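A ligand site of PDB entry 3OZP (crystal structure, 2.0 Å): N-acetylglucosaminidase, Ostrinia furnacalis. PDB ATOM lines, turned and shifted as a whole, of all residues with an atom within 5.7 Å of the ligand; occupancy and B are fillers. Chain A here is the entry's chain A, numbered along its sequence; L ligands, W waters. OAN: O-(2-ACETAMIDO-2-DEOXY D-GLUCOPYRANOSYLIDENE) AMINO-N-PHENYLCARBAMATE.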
ATOM      1  N   ASP A 195     -15.270 -11.054 -34.804  1.00  0.00           N
ATOM      2  CA  ASP A 195     -16.025 -10.689 -33.618  1.00  0.00           C
ATOM      3  C   ASP A 195     -17.495 -11.009 -33.911  1.00  0.00           C
ATOM      4  O   ASP A 195     -18.099 -10.393 -34.782  1.00  0.00           O
ATOM      5  CB  ASP A 195     -15.774  -9.203 -33.331  1.00  0.00           C
ATOM      6  CG  ASP A 195     -16.758  -8.586 -32.337  1.00  0.00           C
ATOM      7  OD1 ASP A 195     -16.696  -7.344 -32.188  1.00  0.00           O
ATOM      8  OD2 ASP A 195     -17.561  -9.292 -31.695  1.00  0.00           O
ATOM      9  N   ARG A 198     -20.411  -8.427 -31.034  1.00  0.00           N
ATOM     10  CA  ARG A 198     -20.900  -7.078 -31.272  1.00  0.00           C
ATOM     11  C   ARG A 198     -22.028  -7.078 -32.302  1.00  0.00           C
ATOM     12  O   ARG A 198     -22.882  -6.207 -32.288  1.00  0.00           O
ATOM     13  CB  ARG A 198     -19.769  -6.135 -31.678  1.00  0.00           C
ATOM     14  CG  ARG A 198     -19.050  -5.498 -30.494  1.00  0.00           C
ATOM     15  CD  ARG A 198     -18.478  -6.522 -29.484  1.00  0.00           C
ATOM     16  NE  ARG A 198     -17.671  -5.820 -28.485  1.00  0.00           N
ATOM     17  CZ  ARG A 198     -16.380  -5.523 -28.639  1.00  0.00           C
ATOM     18  NH1 ARG A 198     -15.728  -5.908 -29.739  1.00  0.00           N
ATOM     19  NH2 ARG A 198     -15.739  -4.855 -27.687  1.00  0.00           N
ATOM     20  N   HIS A 224     -13.831 -14.536 -31.924  1.00  0.00           N
ATOM     21  CA  HIS A 224     -14.101 -13.728 -30.751  1.00  0.00           C
ATOM     22  C   HIS A 224     -15.598 -13.808 -30.488  1.00  0.00           C
ATOM     23  O   HIS A 224     -16.382 -12.964 -30.950  1.00  0.00           O
ATOM     24  CB  HIS A 224     -13.643 -12.288 -30.991  1.00  0.00           C
ATOM     25  CG  HIS A 224     -13.809 -11.384 -29.805  1.00  0.00           C
ATOM     26  ND1 HIS A 224     -12.795 -11.159 -28.898  1.00  0.00           N
ATOM     27  CD2 HIS A 224     -14.856 -10.631 -29.391  1.00  0.00           C
ATOM     28  CE1 HIS A 224     -13.214 -10.310 -27.971  1.00  0.00           C
ATOM     29  NE2 HIS A 224     -14.461  -9.973 -28.253  1.00  0.00           N
ATOM     30  N   ASP A 227     -18.674 -11.092 -25.812  1.00  0.00           N
ATOM     31  CA  ASP A 227     -18.233  -9.785 -25.343  1.00  0.00           C
ATOM     32  C   ASP A 227     -19.338  -9.234 -24.456  1.00  0.00           C
ATOM     33  O   ASP A 227     -20.265  -9.960 -24.100  1.00  0.00           O
ATOM     34  CB  ASP A 227     -17.896  -8.833 -26.501  1.00  0.00           C
ATOM     35  CG  ASP A 227     -16.764  -7.879 -26.157  1.00  0.00           C
ATOM     36  OD1 ASP A 227     -17.001  -6.922 -25.381  1.00  0.00           O
ATOM     37  OD2 ASP A 227     -15.638  -8.080 -26.672  1.00  0.00           O
ATOM     38  N   ASP A 277     -13.025 -13.722 -23.957  1.00  0.00           N
ATOM     39  CA  ASP A 277     -12.432 -12.501 -23.438  1.00  0.00           C
ATOM     40  C   ASP A 277     -12.797 -12.289 -21.963  1.00  0.00           C
ATOM     41  O   ASP A 277     -13.981 -12.269 -21.600  1.00  0.00           O
ATOM     42  CB  ASP A 277     -12.885 -11.319 -24.278  1.00  0.00           C
ATOM     43  CG  ASP A 277     -11.991 -10.112 -24.124  1.00  0.00           C
ATOM     44  OD1 ASP A 277     -12.090  -9.194 -24.962  1.00  0.00           O
ATOM     45  OD2 ASP A 277     -11.179 -10.080 -23.169  1.00  0.00           O
ATOM     46  N   HIS A 281     -14.927  -6.960 -20.973  1.00  0.00           N
ATOM     47  CA  HIS A 281     -15.679  -7.400 -22.156  1.00  0.00           C
ATOM     48  C   HIS A 281     -16.613  -8.571 -21.831  1.00  0.00           C
ATOM     49  O   HIS A 281     -16.673  -9.570 -22.540  1.00  0.00           O
ATOM     50  CB  HIS A 281     -14.719  -7.732 -23.297  1.00  0.00           C
ATOM     51  CG  HIS A 281     -14.013  -6.525 -23.843  1.00  0.00           C
ATOM     52  ND1 HIS A 281     -14.601  -5.669 -24.740  1.00  0.00           N
ATOM     53  CD2 HIS A 281     -12.790  -6.016 -23.570  1.00  0.00           C
ATOM     54  CE1 HIS A 281     -13.759  -4.685 -25.021  1.00  0.00           C
ATOM     55  NE2 HIS A 281     -12.655  -4.876 -24.326  1.00  0.00           N
ATOM     56  N   VAL A 305     -14.128   1.626 -22.142  1.00  0.00           N
ATOM     57  CA  VAL A 305     -13.770   2.266 -23.416  1.00  0.00           C
ATOM     58  C   VAL A 305     -14.927   2.289 -24.445  1.00  0.00           C
ATOM     59  O   VAL A 305     -14.951   3.154 -25.321  1.00  0.00           O
ATOM     60  CB  VAL A 305     -12.387   1.782 -23.997  1.00  0.00           C
ATOM     61  CG1 VAL A 305     -11.818   0.602 -23.208  1.00  0.00           C
ATOM     62  CG2 VAL A 305     -12.429   1.502 -25.507  1.00  0.00           C
ATOM     63  N   GLU A 306     -15.879   1.364 -24.306  1.00  0.00           N
ATOM     64  CA  GLU A 306     -17.099   1.377 -25.126  1.00  0.00           C
ATOM     65  C   GLU A 306     -18.286   0.730 -24.411  1.00  0.00           C
ATOM     66  O   GLU A 306     -18.103  -0.216 -23.647  1.00  0.00           O
ATOM     67  CB  GLU A 306     -16.851   0.712 -26.497  1.00  0.00           C
ATOM     68  CG  GLU A 306     -16.939  -0.800 -26.500  1.00  0.00           C
ATOM     69  CD  GLU A 306     -16.484  -1.401 -27.825  1.00  0.00           C
ATOM     70  OE1 GLU A 306     -17.354  -1.900 -28.577  1.00  0.00           O
ATOM     71  OE2 GLU A 306     -15.271  -1.373 -28.102  1.00  0.00           O
ATOM     72  N   ASP A 345      -7.931  -7.751 -22.769  1.00  0.00           N
ATOM     73  CA  ASP A 345      -7.804  -6.372 -23.221  1.00  0.00           C
ATOM     74  C   ASP A 345      -8.594  -5.421 -22.322  1.00  0.00           C
ATOM     75  O   ASP A 345      -9.691  -5.752 -21.868  1.00  0.00           O
ATOM     76  CB  ASP A 345      -8.230  -6.204 -24.695  1.00  0.00           C
ATOM     77  CG  ASP A 345      -9.652  -6.677 -24.971  1.00  0.00           C
ATOM     78  OD1 ASP A 345     -10.086  -7.677 -24.364  1.00  0.00           O
ATOM     79  OD2 ASP A 345     -10.343  -6.060 -25.802  1.00  0.00           O
ATOM     80  N   GLU A 346      -7.992  -4.258 -22.048  1.00  0.00           N
ATOM     81  CA  GLU A 346      -8.706  -3.078 -21.535  1.00  0.00           C
ATOM     82  C   GLU A 346      -9.457  -3.253 -20.215  1.00  0.00           C
ATOM     83  O   GLU A 346     -10.630  -2.852 -20.102  1.00  0.00           O
ATOM     84  CB  GLU A 346      -9.640  -2.536 -22.613  1.00  0.00           C
ATOM     85  CG  GLU A 346      -8.947  -2.265 -23.942  1.00  0.00           C
ATOM     86  CD  GLU A 346      -9.919  -1.916 -25.047  1.00  0.00           C
ATOM     87  OE1 GLU A 346     -11.000  -2.536 -25.137  1.00  0.00           O
ATOM     88  OE2 GLU A 346      -9.583  -1.011 -25.821  1.00  0.00           O
ATOM     89  N   TRP A 402      -4.196 -10.179 -25.272  1.00  0.00           N
ATOM     90  CA  TRP A 402      -3.964  -8.924 -25.983  1.00  0.00           C
ATOM     91  C   TRP A 402      -2.923  -8.093 -25.239  1.00  0.00           C
ATOM     92  O   TRP A 402      -2.768  -8.231 -24.019  1.00  0.00           O
ATOM     93  CB  TRP A 402      -5.259  -8.104 -26.060  1.00  0.00           C
ATOM     94  CG  TRP A 402      -6.357  -8.737 -26.845  1.00  0.00           C
ATOM     95  CD1 TRP A 402      -7.461  -9.371 -26.349  1.00  0.00           C
ATOM     96  CD2 TRP A 402      -6.475  -8.795 -28.274  1.00  0.00           C
ATOM     97  NE1 TRP A 402      -8.251  -9.810 -27.375  1.00  0.00           N
ATOM     98  CE2 TRP A 402      -7.665  -9.476 -28.560  1.00  0.00           C
ATOM     99  CE3 TRP A 402      -5.683  -8.325 -29.325  1.00  0.00           C
ATOM    100  CZ2 TRP A 402      -8.090  -9.717 -29.874  1.00  0.00           C
ATOM    101  CZ3 TRP A 402      -6.098  -8.561 -30.627  1.00  0.00           C
ATOM    102  CH2 TRP A 402      -7.295  -9.253 -30.884  1.00  0.00           C
ATOM    103  N   TRP A 426      -1.795  -5.256 -30.722  1.00  0.00           N
ATOM    104  CA  TRP A 426      -2.683  -4.385 -31.483  1.00  0.00           C
ATOM    105  C   TRP A 426      -2.332  -2.903 -31.325  1.00  0.00           C
ATOM    106  O   TRP A 426      -3.100  -2.034 -31.723  1.00  0.00           O
ATOM    107  CB  TRP A 426      -4.159  -4.662 -31.144  1.00  0.00           C
ATOM    108  CG  TRP A 426      -4.545  -4.297 -29.742  1.00  0.00           C
ATOM    109  CD1 TRP A 426      -4.265  -5.003 -28.616  1.00  0.00           C
ATOM    110  CD2 TRP A 426      -5.278  -3.139 -29.325  1.00  0.00           C
ATOM    111  NE1 TRP A 426      -4.777  -4.367 -27.513  1.00  0.00           N
ATOM    112  CE2 TRP A 426      -5.407  -3.219 -27.918  1.00  0.00           C
ATOM    113  CE3 TRP A 426      -5.831  -2.053 -30.003  1.00  0.00           C
ATOM    114  CZ2 TRP A 426      -6.068  -2.240 -27.179  1.00  0.00           C
ATOM    115  CZ3 TRP A 426      -6.492  -1.074 -29.264  1.00  0.00           C
ATOM    116  CH2 TRP A 426      -6.612  -1.185 -27.861  1.00  0.00           C
ATOM    117  N   TYR A 453      -6.463  -3.384 -38.592  1.00  0.00           N
ATOM    118  CA  TYR A 453      -7.821  -3.252 -38.059  1.00  0.00           C
ATOM    119  C   TYR A 453      -8.787  -2.940 -39.202  1.00  0.00           C
ATOM    120  O   TYR A 453      -8.881  -1.806 -39.682  1.00  0.00           O
ATOM    121  CB  TYR A 453      -7.866  -2.210 -36.930  1.00  0.00           C
ATOM    122  CG  TYR A 453      -7.683  -2.811 -35.553  1.00  0.00           C
ATOM    123  CD1 TYR A 453      -8.402  -2.345 -34.457  1.00  0.00           C
ATOM    124  CD2 TYR A 453      -6.796  -3.878 -35.349  1.00  0.00           C
ATOM    125  CE1 TYR A 453      -8.235  -2.897 -33.189  1.00  0.00           C
ATOM    126  CE2 TYR A 453      -6.622  -4.444 -34.100  1.00  0.00           C
ATOM    127  CZ  TYR A 453      -7.342  -3.947 -33.023  1.00  0.00           C
ATOM    128  OH  TYR A 453      -7.178  -4.519 -31.785  1.00  0.00           O
ATOM    129  N   ASP A 455     -11.932  -2.877 -39.389  1.00  0.00           N
ATOM    130  CA  ASP A 455     -13.146  -2.149 -39.041  1.00  0.00           C
ATOM    131  C   ASP A 455     -12.999  -0.633 -39.183  1.00  0.00           C
ATOM    132  O   ASP A 455     -14.015   0.086 -39.247  1.00  0.00           O
ATOM    133  CB  ASP A 455     -13.583  -2.524 -37.611  1.00  0.00           C
ATOM    134  CG  ASP A 455     -12.506  -2.266 -36.564  1.00  0.00           C
ATOM    135  OD1 ASP A 455     -11.312  -2.585 -36.818  1.00  0.00           O
ATOM    136  OD2 ASP A 455     -12.833  -1.753 -35.484  1.00  0.00           O
ATOM    137  N   TRP A 468     -13.032   5.259 -34.365  1.00  0.00           N
ATOM    138  CA  TRP A 468     -11.806   5.658 -33.638  1.00  0.00           C
ATOM    139  C   TRP A 468     -10.497   5.520 -34.400  1.00  0.00           C
ATOM    140  O   TRP A 468      -9.595   6.354 -34.247  1.00  0.00           O
ATOM    141  CB  TRP A 468     -11.708   4.942 -32.285  1.00  0.00           C
ATOM    142  CG  TRP A 468     -11.156   3.535 -32.351  1.00  0.00           C
ATOM    143  CD1 TRP A 468     -11.861   2.379 -32.549  1.00  0.00           C
ATOM    144  CD2 TRP A 468      -9.782   3.132 -32.215  1.00  0.00           C
ATOM    145  NE1 TRP A 468     -11.022   1.294 -32.547  1.00  0.00           N
ATOM    146  CE2 TRP A 468      -9.736   1.731 -32.343  1.00  0.00           C
ATOM    147  CE3 TRP A 468      -8.578   3.832 -32.000  1.00  0.00           C
ATOM    148  CZ2 TRP A 468      -8.538   1.004 -32.262  1.00  0.00           C
ATOM    149  CZ3 TRP A 468      -7.389   3.114 -31.915  1.00  0.00           C
ATOM    150  CH2 TRP A 468      -7.385   1.709 -32.052  1.00  0.00           C
ATOM    151  N   CYS A 469     -10.375   4.458 -35.193  1.00  0.00           N
ATOM    152  CA  CYS A 469      -9.103   4.130 -35.840  1.00  0.00           C
ATOM    153  C   CYS A 469      -9.082   4.482 -37.328  1.00  0.00           C
ATOM    154  O   CYS A 469      -8.203   4.034 -38.066  1.00  0.00           O
ATOM    155  CB  CYS A 469      -8.717   2.663 -35.592  1.00  0.00           C
ATOM    156  SG  CYS A 469      -9.926   1.426 -36.153  1.00  0.00           S
ATOM    157  N   TRP A 502     -13.441  -6.411 -35.960  1.00  0.00           N
ATOM    158  CA  TRP A 502     -14.346  -6.066 -34.882  1.00  0.00           C
ATOM    159  C   TRP A 502     -15.681  -5.690 -35.513  1.00  0.00           C
ATOM    160  O   TRP A 502     -15.728  -5.215 -36.648  1.00  0.00           O
ATOM    161  CB  TRP A 502     -13.761  -4.919 -34.067  1.00  0.00           C
ATOM    162  CG  TRP A 502     -12.450  -5.300 -33.470  1.00  0.00           C
ATOM    163  CD1 TRP A 502     -11.215  -4.880 -33.872  1.00  0.00           C
ATOM    164  CD2 TRP A 502     -12.221  -6.222 -32.391  1.00  0.00           C
ATOM    165  NE1 TRP A 502     -10.237  -5.467 -33.101  1.00  0.00           N
ATOM    166  CE2 TRP A 502     -10.831  -6.295 -32.189  1.00  0.00           C
ATOM    167  CE3 TRP A 502     -13.072  -6.990 -31.577  1.00  0.00           C
ATOM    168  CZ2 TRP A 502     -10.253  -7.096 -31.190  1.00  0.00           C
ATOM    169  CZ3 TRP A 502     -12.505  -7.796 -30.591  1.00  0.00           C
ATOM    170  CH2 TRP A 502     -11.106  -7.829 -30.404  1.00  0.00           C
ATOM    171  N   SER A 503     -16.763  -5.936 -34.782  1.00  0.00           N
ATOM    172  CA  SER A 503     -18.072  -5.983 -35.426  1.00  0.00           C
ATOM    173  C   SER A 503     -19.099  -5.012 -34.863  1.00  0.00           C
ATOM    174  O   SER A 503     -20.303  -5.241 -35.003  1.00  0.00           O
ATOM    175  CB  SER A 503     -18.598  -7.415 -35.419  1.00  0.00           C
ATOM    176  OG  SER A 503     -17.710  -8.265 -36.137  1.00  0.00           O
ATOM    177  N   GLU A 504     -18.634  -3.918 -34.260  1.00  0.00           N
ATOM    178  CA  GLU A 504     -19.542  -2.847 -33.869  1.00  0.00           C
ATOM    179  C   GLU A 504     -20.308  -2.352 -35.089  1.00  0.00           C
ATOM    180  O   GLU A 504     -21.459  -1.911 -34.970  1.00  0.00           O
ATOM    181  CB  GLU A 504     -18.799  -1.690 -33.203  1.00  0.00           C
ATOM    182  CG  GLU A 504     -18.234  -2.014 -31.818  1.00  0.00           C
ATOM    183  CD  GLU A 504     -16.809  -2.588 -31.849  1.00  0.00           C
ATOM    184  OE1 GLU A 504     -16.318  -2.941 -32.947  1.00  0.00           O
ATOM    185  OE2 GLU A 504     -16.193  -2.683 -30.773  1.00  0.00           O
HETATM  186  CAH OAN L   1      -8.033  -5.411 -28.377  1.00  0.00           C
HETATM  187  CAG OAN L   1      -9.081  -4.457 -28.926  1.00  0.00           C
HETATM  188  OAN OAN L   1      -9.013  -4.053 -30.088  1.00  0.00           O
HETATM  189  NAI OAN L   1     -10.043  -4.107 -28.050  1.00  0.00           N
HETATM  190  CAB OAN L   1     -11.186  -3.210 -28.377  1.00  0.00           C
HETATM  191  CAC OAN L   1     -12.219  -4.060 -29.152  1.00  0.00           C
HETATM  192  OAJ OAN L   1     -13.118  -4.682 -28.237  1.00  0.00           O
HETATM  193  CAD OAN L   1     -12.985  -3.208 -30.137  1.00  0.00           C
HETATM  194  OAK OAN L   1     -13.960  -4.001 -30.825  1.00  0.00           O
HETATM  195  CAE OAN L   1     -11.962  -2.650 -31.099  1.00  0.00           C
HETATM  196  CAF OAN L   1     -12.638  -1.833 -32.193  1.00  0.00           C
HETATM  197  OAM OAN L   1     -11.652  -1.338 -33.104  1.00  0.00           O
HETATM  198  OAL OAN L   1     -11.052  -1.781 -30.373  1.00  0.00           O
HETATM  199  CAA OAN L   1     -10.751  -2.030 -29.047  1.00  0.00           C
HETATM  200  NAY OAN L   1     -10.034  -1.157 -28.350  1.00  0.00           N
HETATM  201  OAQ OAN L   1      -9.554   0.037 -29.083  1.00  0.00           O
HETATM  202  CAP OAN L   1      -9.810   1.252 -28.498  1.00  0.00           C
HETATM  203  OAR OAN L   1      -9.536   1.450 -27.313  1.00  0.00           O
HETATM  204  NAO OAN L   1     -10.305   2.219 -29.287  1.00  0.00           N
HETATM  205  CAS OAN L   1     -10.583   3.454 -28.867  1.00  0.00           C
HETATM  206  CAT OAN L   1      -9.560   4.404 -28.748  1.00  0.00           C
HETATM  207  CAU OAN L   1      -9.856   5.707 -28.330  1.00  0.00           C
HETATM  208  CAV OAN L   1     -11.177   6.057 -28.053  1.00  0.00           C
HETATM  209  CAW OAN L   1     -12.201   5.120 -28.178  1.00  0.00           C
HETATM  210  CAX OAN L   1     -11.905   3.818 -28.596  1.00  0.00           C
HETATM  211  O   HOH W   1     -14.959   2.766 -28.721  1.00  0.00           O
HETATM  212  O   HOH W   2     -13.668   5.647 -25.197  1.00  0.00           O
HETATM  213  O   HOH W   3      -8.858   4.563 -25.256  1.00  0.00           O
HETATM  214  O   HOH W   4     -15.245   5.090 -29.671  1.00  0.00           O
HETATM  215  O   HOH W   5     -12.720  -6.926 -27.161  1.00  0.00           O
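OH of Tyr 453 lies within hydrogen-bond range of OAN of the ligand (2.5 Å). OE2 of Glu 346 sits at hydrogen-bond distance from NAY of the ligand, 2.6 Å away. An oxygen (OAK) of the ligand is in hydrogen-bond range of the side-chain carboxylate of Glu 504 (2.6 Å). An oxygen (OAJ) of the ligand sits at hydrogen-bond distance from the guanidinium group of Arg 198, at 2.7 Å. An oxygen (OAM) of the ligand is in hydrogen-bond range of the side-chain carboxylate (OD2) of Asp 455. An oxygen (OAM) of the ligand sits at hydrogen-bond distance from the indole nitrogen (NE1) of Trp 468 (2.8 Å). NAI of the ligand is in hydrogen-bond range of OD2 of Asp 345 (3.0 Å).
OE2 of Glu 504 is in salt-bridge range of NH1 of Arg 198. The guanidinium group (NH2) of Arg 198 sits at hydrogen-bond distance from a ring nitrogen (ND1) of His 281 (3.3 Å). The side-chain carboxylate of Glu 306 lies within salt-bridge range of the guanidinium group of Arg 198, 3.5 Å away. The side-chain carboxylate of Asp 227 lies within salt-bridge range of the guanidinium group of Arg 198 (3.3 Å). OD1 of Asp 195 lies within salt-bridge range of NH1 of Arg 198 (3.0 Å). OD2 of Asp 345 is in hydrogen-bond range of NE2 of His 281 (3.0 Å). The side-chain carboxylate of Asp 345 sits close to the side-chain carboxylate of Asp 277 (2.6 Å). OD1 of Asp 227 is in hydrogen-bond range of ND1 of His 281, 2.8 Å away.
CE1 of His 281 touches OAJ of the ligand, at 3.3 Å. CG2 of Val 305 touches OAR of the ligand (3.4 Å). Glu 306 touches the ligand. Trp 402 touches the ligand (CD2 to CAH, 3.7 Å). Trp 426 touches the ligand. Trp 502 touches the ligand. Hydrophobic or aromatic side chains that line the ligand: His 281, Val 305, Trp 402, Trp 426, Tyr 453, Trp 468 and Trp 502. Within 4 Å of the ligand: Arg 198, His 281, Val 305, Glu 306, Asp 345, Glu 346, Trp 402, Trp 426, Tyr 453, Asp 455, Trp 468, Trp 502 and Glu 504.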
